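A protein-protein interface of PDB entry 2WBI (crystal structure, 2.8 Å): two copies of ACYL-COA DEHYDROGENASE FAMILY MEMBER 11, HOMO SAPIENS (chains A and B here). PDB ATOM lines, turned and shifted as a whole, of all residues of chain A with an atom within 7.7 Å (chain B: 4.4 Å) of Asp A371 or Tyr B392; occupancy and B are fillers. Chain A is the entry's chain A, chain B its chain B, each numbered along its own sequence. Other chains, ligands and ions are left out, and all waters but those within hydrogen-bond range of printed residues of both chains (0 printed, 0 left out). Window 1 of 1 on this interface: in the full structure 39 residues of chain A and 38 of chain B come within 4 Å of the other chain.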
ATOM      1  N   PHE A 236      -7.609  16.951  -3.352  1.00  0.00           N
ATOM      2  CA  PHE A 236      -6.747  16.761  -2.180  1.00  0.00           C
ATOM      3  C   PHE A 236      -7.369  15.790  -1.152  1.00  0.00           C
ATOM      4  O   PHE A 236      -7.389  16.055   0.041  1.00  0.00           O
ATOM      5  CB  PHE A 236      -6.416  18.084  -1.499  1.00  0.00           C
ATOM      6  CG  PHE A 236      -5.799  19.084  -2.396  1.00  0.00           C
ATOM      7  CD1 PHE A 236      -4.463  19.011  -2.730  1.00  0.00           C
ATOM      8  CD2 PHE A 236      -6.543  20.130  -2.900  1.00  0.00           C
ATOM      9  CE1 PHE A 236      -3.887  19.967  -3.576  1.00  0.00           C
ATOM     10  CE2 PHE A 236      -5.963  21.083  -3.731  1.00  0.00           C
ATOM     11  CZ  PHE A 236      -4.644  20.993  -4.070  1.00  0.00           C
ATOM     12  N   ALA A 294     -12.569  33.917   5.665  1.00  0.00           N
ATOM     13  CA  ALA A 294     -11.162  33.651   5.931  1.00  0.00           C
ATOM     14  C   ALA A 294     -10.483  34.774   6.717  1.00  0.00           C
ATOM     15  O   ALA A 294      -9.764  34.516   7.691  1.00  0.00           O
ATOM     16  CB  ALA A 294     -10.427  33.405   4.651  1.00  0.00           C
ATOM     17  N   MET A 298      -8.877  34.741  10.354  1.00  0.00           N
ATOM     18  CA  MET A 298      -7.492  35.204  10.501  1.00  0.00           C
ATOM     19  C   MET A 298      -7.298  36.222  11.626  1.00  0.00           C
ATOM     20  O   MET A 298      -6.298  36.181  12.345  1.00  0.00           O
ATOM     21  CB  MET A 298      -7.000  35.804   9.184  1.00  0.00           C
ATOM     22  CG  MET A 298      -5.505  35.973   9.100  1.00  0.00           C
ATOM     23  SD  MET A 298      -4.940  37.019   7.737  1.00  0.00           S
ATOM     24  CE  MET A 298      -5.530  36.143   6.290  1.00  0.00           C
ATOM     25  N   TRP A 321      -0.346  40.907   6.195  1.00  0.00           N
ATOM     26  CA  TRP A 321      -1.245  39.943   5.552  1.00  0.00           C
ATOM     27  C   TRP A 321      -2.709  40.356   5.733  1.00  0.00           C
ATOM     28  O   TRP A 321      -3.501  40.288   4.792  1.00  0.00           O
ATOM     29  CB  TRP A 321      -1.050  38.530   6.113  1.00  0.00           C
ATOM     30  CG  TRP A 321       0.303  37.929   5.914  1.00  0.00           C
ATOM     31  CD1 TRP A 321       1.245  38.302   5.009  1.00  0.00           C
ATOM     32  CD2 TRP A 321       0.841  36.798   6.607  1.00  0.00           C
ATOM     33  NE1 TRP A 321       2.351  37.500   5.113  1.00  0.00           N
ATOM     34  CE2 TRP A 321       2.127  36.560   6.086  1.00  0.00           C
ATOM     35  CE3 TRP A 321       0.363  35.967   7.624  1.00  0.00           C
ATOM     36  CZ2 TRP A 321       2.946  35.515   6.549  1.00  0.00           C
ATOM     37  CZ3 TRP A 321       1.179  34.934   8.091  1.00  0.00           C
ATOM     38  CH2 TRP A 321       2.452  34.718   7.550  1.00  0.00           C
ATOM     39  N   ALA A 365      -6.590  35.247  -5.999  1.00  0.00           N
ATOM     40  CA  ALA A 365      -6.447  36.200  -4.914  1.00  0.00           C
ATOM     41  C   ALA A 365      -6.954  35.599  -3.607  1.00  0.00           C
ATOM     42  O   ALA A 365      -6.277  35.662  -2.571  1.00  0.00           O
ATOM     43  CB  ALA A 365      -7.178  37.489  -5.232  1.00  0.00           C
ATOM     44  N   VAL A 366      -8.142  35.012  -3.658  1.00  0.00           N
ATOM     45  CA  VAL A 366      -8.776  34.488  -2.457  1.00  0.00           C
ATOM     46  C   VAL A 366      -8.009  33.266  -1.958  1.00  0.00           C
ATOM     47  O   VAL A 366      -7.865  33.061  -0.754  1.00  0.00           O
ATOM     48  CB  VAL A 366     -10.273  34.167  -2.715  1.00  0.00           C
ATOM     49  CG1 VAL A 366     -10.900  33.416  -1.557  1.00  0.00           C
ATOM     50  CG2 VAL A 366     -11.011  35.449  -2.960  1.00  0.00           C
ATOM     51  N   SER A 367      -7.515  32.478  -2.906  1.00  0.00           N
ATOM     52  CA  SER A 367      -6.616  31.359  -2.629  1.00  0.00           C
ATOM     53  C   SER A 367      -5.448  31.776  -1.736  1.00  0.00           C
ATOM     54  O   SER A 367      -5.114  31.087  -0.774  1.00  0.00           O
ATOM     55  CB  SER A 367      -6.071  30.842  -3.948  1.00  0.00           C
ATOM     56  OG  SER A 367      -5.726  29.493  -3.829  1.00  0.00           O
ATOM     57  N   LYS A 368      -4.852  32.921  -2.069  1.00  0.00           N
ATOM     58  CA  LYS A 368      -3.729  33.496  -1.347  1.00  0.00           C
ATOM     59  C   LYS A 368      -4.146  33.932   0.065  1.00  0.00           C
ATOM     60  O   LYS A 368      -3.422  33.698   1.036  1.00  0.00           O
ATOM     61  CB  LYS A 368      -3.162  34.655  -2.145  1.00  0.00           C
ATOM     62  CG  LYS A 368      -1.821  35.141  -1.653  1.00  0.00           C
ATOM     63  CD  LYS A 368      -1.270  36.279  -2.561  1.00  0.00           C
ATOM     64  CE  LYS A 368       0.172  36.696  -2.166  1.00  0.00           C
ATOM     65  NZ  LYS A 368       0.589  38.001  -2.796  1.00  0.00           N
ATOM     66  N   ILE A 369      -5.316  34.552   0.176  1.00  0.00           N
ATOM     67  CA  ILE A 369      -5.882  34.925   1.477  1.00  0.00           C
ATOM     68  C   ILE A 369      -6.111  33.713   2.384  1.00  0.00           C
ATOM     69  O   ILE A 369      -5.776  33.729   3.565  1.00  0.00           O
ATOM     70  CB  ILE A 369      -7.197  35.733   1.316  1.00  0.00           C
ATOM     71  CG1 ILE A 369      -6.894  37.091   0.666  1.00  0.00           C
ATOM     72  CG2 ILE A 369      -7.872  35.924   2.660  1.00  0.00           C
ATOM     73  CD1 ILE A 369      -8.113  37.875   0.163  1.00  0.00           C
ATOM     74  N   VAL A 370      -6.681  32.661   1.824  1.00  0.00           N
ATOM     75  CA  VAL A 370      -6.936  31.458   2.586  1.00  0.00           C
ATOM     76  C   VAL A 370      -5.609  30.888   3.069  1.00  0.00           C
ATOM     77  O   VAL A 370      -5.490  30.514   4.228  1.00  0.00           O
ATOM     78  CB  VAL A 370      -7.716  30.440   1.759  1.00  0.00           C
ATOM     79  CG1 VAL A 370      -7.889  29.137   2.536  1.00  0.00           C
ATOM     80  CG2 VAL A 370      -9.062  31.029   1.395  1.00  0.00           C
ATOM     81  N   ASP A 371      -4.610  30.860   2.187  1.00  0.00           N
ATOM     82  CA  ASP A 371      -3.289  30.307   2.519  1.00  0.00           C
ATOM     83  C   ASP A 371      -2.528  31.064   3.621  1.00  0.00           C
ATOM     84  O   ASP A 371      -1.781  30.464   4.393  1.00  0.00           O
ATOM     85  CB  ASP A 371      -2.405  30.233   1.284  1.00  0.00           C
ATOM     86  CG  ASP A 371      -1.163  29.407   1.523  1.00  0.00           C
ATOM     87  OD1 ASP A 371      -1.285  28.169   1.694  1.00  0.00           O
ATOM     88  OD2 ASP A 371      -0.073  30.006   1.560  1.00  0.00           O
ATOM     89  N   TRP A 372      -2.698  32.378   3.666  1.00  0.00           N
ATOM     90  CA  TRP A 372      -2.170  33.172   4.761  1.00  0.00           C
ATOM     91  C   TRP A 372      -2.941  32.895   6.022  1.00  0.00           C
ATOM     92  O   TRP A 372      -2.354  32.862   7.094  1.00  0.00           O
ATOM     93  CB  TRP A 372      -2.314  34.655   4.482  1.00  0.00           C
ATOM     94  CG  TRP A 372      -1.302  35.260   3.584  1.00  0.00           C
ATOM     95  CD1 TRP A 372      -0.006  34.865   3.413  1.00  0.00           C
ATOM     96  CD2 TRP A 372      -1.478  36.441   2.780  1.00  0.00           C
ATOM     97  NE1 TRP A 372       0.628  35.703   2.521  1.00  0.00           N
ATOM     98  CE2 TRP A 372      -0.247  36.683   2.121  1.00  0.00           C
ATOM     99  CE3 TRP A 372      -2.564  37.312   2.540  1.00  0.00           C
ATOM    100  CZ2 TRP A 372      -0.071  37.753   1.228  1.00  0.00           C
ATOM    101  CZ3 TRP A 372      -2.388  38.374   1.646  1.00  0.00           C
ATOM    102  CH2 TRP A 372      -1.147  38.581   1.005  1.00  0.00           C
ATOM    103  N   ALA A 373      -4.260  32.731   5.895  1.00  0.00           N
ATOM    104  CA  ALA A 373      -5.104  32.418   7.042  1.00  0.00           C
ATOM    105  C   ALA A 373      -4.683  31.076   7.639  1.00  0.00           C
ATOM    106  O   ALA A 373      -4.640  30.918   8.858  1.00  0.00           O
ATOM    107  CB  ALA A 373      -6.569  32.409   6.645  1.00  0.00           C
ATOM    108  N   ILE A 374      -4.341  30.123   6.776  1.00  0.00           N
ATOM    109  CA  ILE A 374      -3.924  28.811   7.226  1.00  0.00           C
ATOM    110  C   ILE A 374      -2.626  28.940   7.999  1.00  0.00           C
ATOM    111  O   ILE A 374      -2.438  28.269   9.026  1.00  0.00           O
ATOM    112  CB  ILE A 374      -3.754  27.845   6.068  1.00  0.00           C
ATOM    113  CG1 ILE A 374      -5.118  27.442   5.544  1.00  0.00           C
ATOM    114  CG2 ILE A 374      -3.030  26.618   6.526  1.00  0.00           C
ATOM    115  CD1 ILE A 374      -5.078  26.894   4.188  1.00  0.00           C
ATOM    116  N   GLN A 375      -1.758  29.829   7.520  1.00  0.00           N
ATOM    117  CA  GLN A 375      -0.434  30.015   8.088  1.00  0.00           C
ATOM    118  C   GLN A 375      -0.520  30.641   9.472  1.00  0.00           C
ATOM    119  O   GLN A 375       0.267  30.315  10.372  1.00  0.00           O
ATOM    120  CB  GLN A 375       0.415  30.880   7.156  1.00  0.00           C
ATOM    121  CG  GLN A 375       1.909  30.946   7.489  1.00  0.00           C
ATOM    122  CD  GLN A 375       2.653  29.624   7.278  1.00  0.00           C
ATOM    123  OE1 GLN A 375       2.210  28.752   6.527  1.00  0.00           O
ATOM    124  NE2 GLN A 375       3.792  29.477   7.946  1.00  0.00           N
ATOM    125  N   VAL A 376      -1.488  31.541   9.633  1.00  0.00           N
ATOM    126  CA  VAL A 376      -1.708  32.233  10.893  1.00  0.00           C
ATOM    127  C   VAL A 376      -2.253  31.246  11.924  1.00  0.00           C
ATOM    128  O   VAL A 376      -1.952  31.354  13.123  1.00  0.00           O
ATOM    129  CB  VAL A 376      -2.661  33.455  10.700  1.00  0.00           C
ATOM    130  CG1 VAL A 376      -3.152  34.035  12.045  1.00  0.00           C
ATOM    131  CG2 VAL A 376      -1.973  34.537   9.904  1.00  0.00           C
ATOM    132  N   CYS A 377      -3.025  30.267  11.447  1.00  0.00           N
ATOM    133  CA  CYS A 377      -3.612  29.254  12.321  1.00  0.00           C
ATOM    134  C   CYS A 377      -2.674  28.113  12.749  1.00  0.00           C
ATOM    135  O   CYS A 377      -3.071  27.241  13.549  1.00  0.00           O
ATOM    136  CB  CYS A 377      -4.892  28.716  11.701  1.00  0.00           C
ATOM    137  SG  CYS A 377      -6.222  29.919  11.814  1.00  0.00           S
ATOM    138  N   VAL A 382      -4.451  23.469   8.606  1.00  0.00           N
ATOM    139  CA  VAL A 382      -4.669  22.343   7.690  1.00  0.00           C
ATOM    140  C   VAL A 382      -5.645  21.294   8.244  1.00  0.00           C
ATOM    141  O   VAL A 382      -6.002  20.324   7.544  1.00  0.00           O
ATOM    142  CB  VAL A 382      -3.336  21.658   7.247  1.00  0.00           C
ATOM    143  CG1 VAL A 382      -2.435  22.663   6.559  1.00  0.00           C
ATOM    144  CG2 VAL A 382      -2.615  20.992   8.417  1.00  0.00           C
ATOM    145  N   LEU A 388     -10.714  26.288   6.838  1.00  0.00           N
ATOM    146  CA  LEU A 388      -9.742  26.865   5.906  1.00  0.00           C
ATOM    147  C   LEU A 388      -9.192  25.885   4.878  1.00  0.00           C
ATOM    148  O   LEU A 388      -9.000  26.261   3.729  1.00  0.00           O
ATOM    149  CB  LEU A 388      -8.582  27.534   6.641  1.00  0.00           C
ATOM    150  CG  LEU A 388      -8.939  28.711   7.560  1.00  0.00           C
ATOM    151  CD1 LEU A 388      -7.802  29.054   8.559  1.00  0.00           C
ATOM    152  CD2 LEU A 388      -9.393  29.949   6.803  1.00  0.00           C
ATOM    153  N   MET A 391     -11.763  25.475   2.308  1.00  0.00           N
ATOM    154  CA  MET A 391     -11.766  26.731   1.562  1.00  0.00           C
ATOM    155  C   MET A 391     -10.587  26.787   0.582  1.00  0.00           C
ATOM    156  O   MET A 391     -10.751  27.188  -0.580  1.00  0.00           O
ATOM    157  CB  MET A 391     -11.778  27.950   2.504  1.00  0.00           C
ATOM    158  CG  MET A 391     -13.113  28.113   3.245  1.00  0.00           C
ATOM    159  SD  MET A 391     -13.075  29.016   4.826  1.00  0.00           S
ATOM    160  CE  MET A 391     -12.449  30.566   4.237  1.00  0.00           C
ATOM    161  N   TYR A 392      -9.410  26.356   1.012  1.00  0.00           N
ATOM    162  CA  TYR A 392      -8.316  26.335   0.068  1.00  0.00           C
ATOM    163  C   TYR A 392      -8.585  25.400  -1.154  1.00  0.00           C
ATOM    164  O   TYR A 392      -8.364  25.795  -2.302  1.00  0.00           O
ATOM    165  CB  TYR A 392      -6.951  26.093   0.729  1.00  0.00           C
ATOM    166  CG  TYR A 392      -5.881  26.109  -0.320  1.00  0.00           C
ATOM    167  CD1 TYR A 392      -5.330  27.312  -0.757  1.00  0.00           C
ATOM    168  CD2 TYR A 392      -5.478  24.927  -0.945  1.00  0.00           C
ATOM    169  CE1 TYR A 392      -4.356  27.331  -1.771  1.00  0.00           C
ATOM    170  CE2 TYR A 392      -4.526  24.929  -1.931  1.00  0.00           C
ATOM    171  CZ  TYR A 392      -3.967  26.125  -2.351  1.00  0.00           C
ATOM    172  OH  TYR A 392      -3.024  26.098  -3.357  1.00  0.00           O
ATOM    173  N   THR A 395     -10.914  27.015  -3.702  1.00  0.00           N
ATOM    174  CA  THR A 395     -10.355  28.095  -4.496  1.00  0.00           C
ATOM    175  C   THR A 395      -9.323  27.581  -5.480  1.00  0.00           C
ATOM    176  O   THR A 395      -9.224  28.085  -6.579  1.00  0.00           O
ATOM    177  CB  THR A 395      -9.775  29.215  -3.616  1.00  0.00           C
ATOM    178  OG1 THR A 395      -8.716  28.698  -2.785  1.00  0.00           O
ATOM    179  CG2 THR A 395     -10.874  29.814  -2.749  1.00  0.00           C
ATOM    180  N   ARG A 396      -8.583  26.553  -5.100  1.00  0.00           N
ATOM    181  CA  ARG A 396      -7.613  25.955  -5.997  1.00  0.00           C
ATOM    182  C   ARG A 396      -8.316  25.403  -7.213  1.00  0.00           C
ATOM    183  O   ARG A 396      -7.821  25.498  -8.319  1.00  0.00           O
ATOM    184  CB  ARG A 396      -6.818  24.836  -5.296  1.00  0.00           C
ATOM    185  CG  ARG A 396      -5.679  24.228  -6.118  1.00  0.00           C
ATOM    186  CD  ARG A 396      -4.709  25.324  -6.562  1.00  0.00           C
ATOM    187  NE  ARG A 396      -3.700  24.864  -7.513  1.00  0.00           N
ATOM    188  CZ  ARG A 396      -3.891  24.736  -8.820  1.00  0.00           C
ATOM    189  NH1 ARG A 396      -5.068  25.015  -9.349  1.00  0.00           N
ATOM    190  NH2 ARG A 396      -2.903  24.322  -9.597  1.00  0.00           N
ATOM    191  N   SER B 367       6.732  23.805  -3.304  1.00  0.00           N
ATOM    192  CA  SER B 367       5.295  24.058  -3.290  1.00  0.00           C
ATOM    193  C   SER B 367       4.755  24.683  -4.599  1.00  0.00           C
ATOM    194  O   SER B 367       3.786  24.201  -5.188  1.00  0.00           O
ATOM    195  CB  SER B 367       5.006  24.995  -2.150  1.00  0.00           C
ATOM    196  OG  SER B 367       3.659  24.902  -1.802  1.00  0.00           O
ATOM    197  N   VAL B 370       5.056  22.228  -7.556  1.00  0.00           N
ATOM    198  CA  VAL B 370       3.995  21.239  -7.493  1.00  0.00           C
ATOM    199  C   VAL B 370       2.659  21.826  -7.958  1.00  0.00           C
ATOM    200  O   VAL B 370       1.921  21.197  -8.722  1.00  0.00           O
ATOM    201  CB  VAL B 370       3.861  20.664  -6.080  1.00  0.00           C
ATOM    202  CG1 VAL B 370       2.700  19.658  -6.015  1.00  0.00           C
ATOM    203  CG2 VAL B 370       5.187  20.018  -5.628  1.00  0.00           C
ATOM    204  N   ILE B 374       0.355  20.664 -11.001  1.00  0.00           N
ATOM    205  CA  ILE B 374      -1.065  20.388 -10.851  1.00  0.00           C
ATOM    206  C   ILE B 374      -1.883  21.068 -11.942  1.00  0.00           C
ATOM    207  O   ILE B 374      -2.763  20.431 -12.552  1.00  0.00           O
ATOM    208  CB  ILE B 374      -1.586  20.816  -9.477  1.00  0.00           C
ATOM    209  CG1 ILE B 374      -1.107  19.826  -8.403  1.00  0.00           C
ATOM    210  CG2 ILE B 374      -3.102  20.858  -9.479  1.00  0.00           C
ATOM    211  CD1 ILE B 374      -1.136  20.349  -6.995  1.00  0.00           C
ATOM    212  N   LEU B 388       0.481  14.333  -7.218  1.00  0.00           N
ATOM    213  CA  LEU B 388       0.773  15.761  -7.054  1.00  0.00           C
ATOM    214  C   LEU B 388       0.026  16.400  -5.883  1.00  0.00           C
ATOM    215  O   LEU B 388       0.582  17.188  -5.112  1.00  0.00           O
ATOM    216  CB  LEU B 388       0.501  16.526  -8.353  1.00  0.00           C
ATOM    217  CG  LEU B 388       1.325  16.155  -9.584  1.00  0.00           C
ATOM    218  CD1 LEU B 388       0.664  16.656 -10.840  1.00  0.00           C
ATOM    219  CD2 LEU B 388       2.719  16.710  -9.442  1.00  0.00           C
ATOM    220  N   ALA B 389      -1.240  16.039  -5.740  1.00  0.00           N
ATOM    221  CA  ALA B 389      -2.066  16.579  -4.658  1.00  0.00           C
ATOM    222  C   ALA B 389      -1.491  16.236  -3.278  1.00  0.00           C
ATOM    223  O   ALA B 389      -1.482  17.082  -2.384  1.00  0.00           O
ATOM    224  CB  ALA B 389      -3.519  16.114  -4.799  1.00  0.00           C
ATOM    225  N   ASN B 390      -1.012  15.001  -3.116  1.00  0.00           N
ATOM    226  CA  ASN B 390      -0.271  14.595  -1.931  1.00  0.00           C
ATOM    227  C   ASN B 390       1.016  15.364  -1.752  1.00  0.00           C
ATOM    228  O   ASN B 390       1.281  15.911  -0.677  1.00  0.00           O
ATOM    229  CB  ASN B 390       0.058  13.133  -2.033  1.00  0.00           C
ATOM    230  CG  ASN B 390      -1.012  12.264  -1.424  1.00  0.00           C
ATOM    231  OD1 ASN B 390      -1.146  12.212  -0.208  1.00  0.00           O
ATOM    232  ND2 ASN B 390      -1.766  11.573  -2.255  1.00  0.00           N
ATOM    233  N   MET B 391       1.807  15.412  -2.825  1.00  0.00           N
ATOM    234  CA  MET B 391       3.039  16.195  -2.860  1.00  0.00           C
ATOM    235  C   MET B 391       2.781  17.634  -2.436  1.00  0.00           C
ATOM    236  O   MET B 391       3.558  18.181  -1.652  1.00  0.00           O
ATOM    237  CB  MET B 391       3.719  16.103  -4.239  1.00  0.00           C
ATOM    238  CG  MET B 391       4.239  14.715  -4.537  1.00  0.00           C
ATOM    239  SD  MET B 391       4.620  14.304  -6.258  1.00  0.00           S
ATOM    240  CE  MET B 391       5.696  15.655  -6.693  1.00  0.00           C
ATOM    241  N   TYR B 392       1.691  18.242  -2.915  1.00  0.00           N
ATOM    242  CA  TYR B 392       1.398  19.620  -2.495  1.00  0.00           C
ATOM    243  C   TYR B 392       1.172  19.726  -0.974  1.00  0.00           C
ATOM    244  O   TYR B 392       1.781  20.555  -0.313  1.00  0.00           O
ATOM    245  CB  TYR B 392       0.274  20.307  -3.315  1.00  0.00           C
ATOM    246  CG  TYR B 392       0.053  21.701  -2.806  1.00  0.00           C
ATOM    247  CD1 TYR B 392       0.885  22.759  -3.199  1.00  0.00           C
ATOM    248  CD2 TYR B 392      -0.917  21.951  -1.846  1.00  0.00           C
ATOM    249  CE1 TYR B 392       0.712  24.031  -2.683  1.00  0.00           C
ATOM    250  CE2 TYR B 392      -1.084  23.194  -1.319  1.00  0.00           C
ATOM    251  CZ  TYR B 392      -0.273  24.244  -1.728  1.00  0.00           C
ATOM    252  OH  TYR B 392      -0.486  25.510  -1.172  1.00  0.00           O
ATOM    253  N   ALA B 393       0.318  18.865  -0.427  1.00  0.00           N
ATOM    254  CA  ALA B 393       0.075  18.790   1.004  1.00  0.00           C
ATOM    255  C   ALA B 393       1.356  18.639   1.821  1.00  0.00           C
ATOM    256  O   ALA B 393       1.490  19.274   2.859  1.00  0.00           O
ATOM    257  CB  ALA B 393      -0.873  17.650   1.299  1.00  0.00           C
ATOM    258  N   ILE B 394       2.292  17.793   1.368  1.00  0.00           N
ATOM    259  CA  ILE B 394       3.555  17.622   2.081  1.00  0.00           C
ATOM    260  C   ILE B 394       4.319  18.941   2.120  1.00  0.00           C
ATOM    261  O   ILE B 394       4.765  19.382   3.183  1.00  0.00           O
ATOM    262  CB  ILE B 394       4.450  16.525   1.491  1.00  0.00           C
ATOM    263  CG1 ILE B 394       3.823  15.140   1.662  1.00  0.00           C
ATOM    264  CG2 ILE B 394       5.820  16.541   2.164  1.00  0.00           C
ATOM    265  CD1 ILE B 394       4.349  14.098   0.655  1.00  0.00           C
ATOM    266  N   THR B 395       4.460  19.595   0.978  1.00  0.00           N
ATOM    267  CA  THR B 395       5.243  20.826   0.969  1.00  0.00           C
ATOM    268  C   THR B 395       4.561  21.935   1.752  1.00  0.00           C
ATOM    269  O   THR B 395       5.226  22.699   2.419  1.00  0.00           O
ATOM    270  CB  THR B 395       5.640  21.301  -0.458  1.00  0.00           C
ATOM    271  OG1 THR B 395       4.470  21.705  -1.191  1.00  0.00           O
ATOM    272  CG2 THR B 395       6.374  20.193  -1.184  1.00  0.00           C
ATOM    273  N   ARG B 396       3.238  22.005   1.693  1.00  0.00           N
ATOM    274  CA  ARG B 396       2.517  23.034   2.427  1.00  0.00           C
ATOM    275  C   ARG B 396       2.806  22.887   3.918  1.00  0.00           C
ATOM    276  O   ARG B 396       3.041  23.874   4.622  1.00  0.00           O
ATOM    277  CB  ARG B 396       1.008  22.976   2.149  1.00  0.00           C
ATOM    278  CG  ARG B 396       0.194  24.086   2.823  1.00  0.00           C
ATOM    279  CD  ARG B 396       0.674  25.445   2.363  1.00  0.00           C
ATOM    280  NE  ARG B 396       0.061  26.578   3.050  1.00  0.00           N
ATOM    281  CZ  ARG B 396       0.498  27.094   4.194  1.00  0.00           C
ATOM    282  NH1 ARG B 396       1.542  26.549   4.803  1.00  0.00           N
ATOM    283  NH2 ARG B 396      -0.118  28.139   4.739  1.00  0.00           N
ATOM    284  N   ARG B 399       6.124  24.238   5.507  1.00  0.00           N
ATOM    285  CA  ARG B 399       6.230  25.665   5.841  1.00  0.00           C
ATOM    286  C   ARG B 399       5.794  25.922   7.279  1.00  0.00           C
ATOM    287  O   ARG B 399       5.945  27.032   7.781  1.00  0.00           O
ATOM    288  CB  ARG B 399       5.414  26.524   4.863  1.00  0.00           C
ATOM    289  CG  ARG B 399       5.761  26.248   3.415  1.00  0.00           C
ATOM    290  CD  ARG B 399       4.865  26.966   2.487  1.00  0.00           C
ATOM    291  NE  ARG B 399       4.633  28.311   2.985  1.00  0.00           N
ATOM    292  CZ  ARG B 399       3.601  29.077   2.641  1.00  0.00           C
ATOM    293  NH1 ARG B 399       2.691  28.627   1.770  1.00  0.00           N
ATOM    294  NH2 ARG B 399       3.476  30.290   3.188  1.00  0.00           N
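Ile A374 touches Arg B396, and with the chains exchanged Arg A396 touches Ile B374.
Tyr A392 touches its own counterpart, Tyr B392.
8 positions are printed for both chains.
Of the 10 pairs that touch across the chains among the printed residues, 3 have their exchanged pair printed and touching as well.
The backbone carbonyl oxygen (O) of Tyr B392 lies within hydrogen-bond range of the side-chain hydroxyl (OG1) of Thr B395 (3.1 Å).
The backbone carbonyl oxygen (O) of Tyr A392 sits at hydrogen-bond distance from the side-chain hydroxyl (OG1) of Thr A395, at 3.0 Å.
Trp A321 touches none of the printed residues of chain B.
Ser A367 touches none of the printed residues of chain B.
Of the printed residues of chain B, Asp A371 touches Tyr B392, Arg B396 and Arg B399.
Of the printed residues of chain B, Gln A375 touches Arg B396 (2.9 Å) and Arg B399 (3.3 Å).
Of the printed residues of chain B, Tyr A392 touches Tyr B392.
Of the printed residues of chain A, Ala B389 touches Phe A236.
Printed residues of chain A within 4 Å of Arg B396: Asp A371 (2.5 Å), Ile A374 (3.7 Å) and Gln A375 (2.9 Å).
Of the printed residues of chain A, Arg B399 touches Asp A371 (3.1 Å) and Gln A375 (3.3 Å).
The nearest printed residue of chain B that does not touch Asp A371 is Ser B367 (6.9 Å).
The nearest printed residue of chain A that does not touch Arg B399 is Trp A372 (5.8 Å).
OH of Tyr B392 sits at hydrogen-bond distance from OH of Tyr A392 (3.4 Å).
NE2 of Gln A375 lies within hydrogen-bond range of O of Arg B399, at 3.3 Å.
NH1 of Arg B399 is in salt-bridge range of OD2 of Asp A371 (3.1 Å).
NH1 of Arg B396 sits at hydrogen-bond distance from OE1 of Gln A375, 2.9 Å away.
OD1 of Asp A371 lies within salt-bridge range of NE of Arg B396 (2.5 Å).
Among the printed residues, merely in contact across the chains: Phe A236 with Ala B389 (3.6 Å), Phe A236 with Tyr B392 (3.97 Å), Asp A371 with Tyr B392 (3.99 Å), Ile A374 with Arg B396 (3.7 Å) and Arg A396 with Ile B374 (3.5 Å).
Hydrophobic or aromatic side chains of chain B that line the printed part of chain A: Ile B374, Ala B389 and Tyr B392.
Hydrophobic or aromatic side chains of chain A that line the printed part of chain B: Phe A236, Ile A374 and Tyr A392.
Along chain A the printed residues that touch a printed residue of chain B span positions 236 to 396.
Among the printed residues, 10 pairs touch across the chains.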
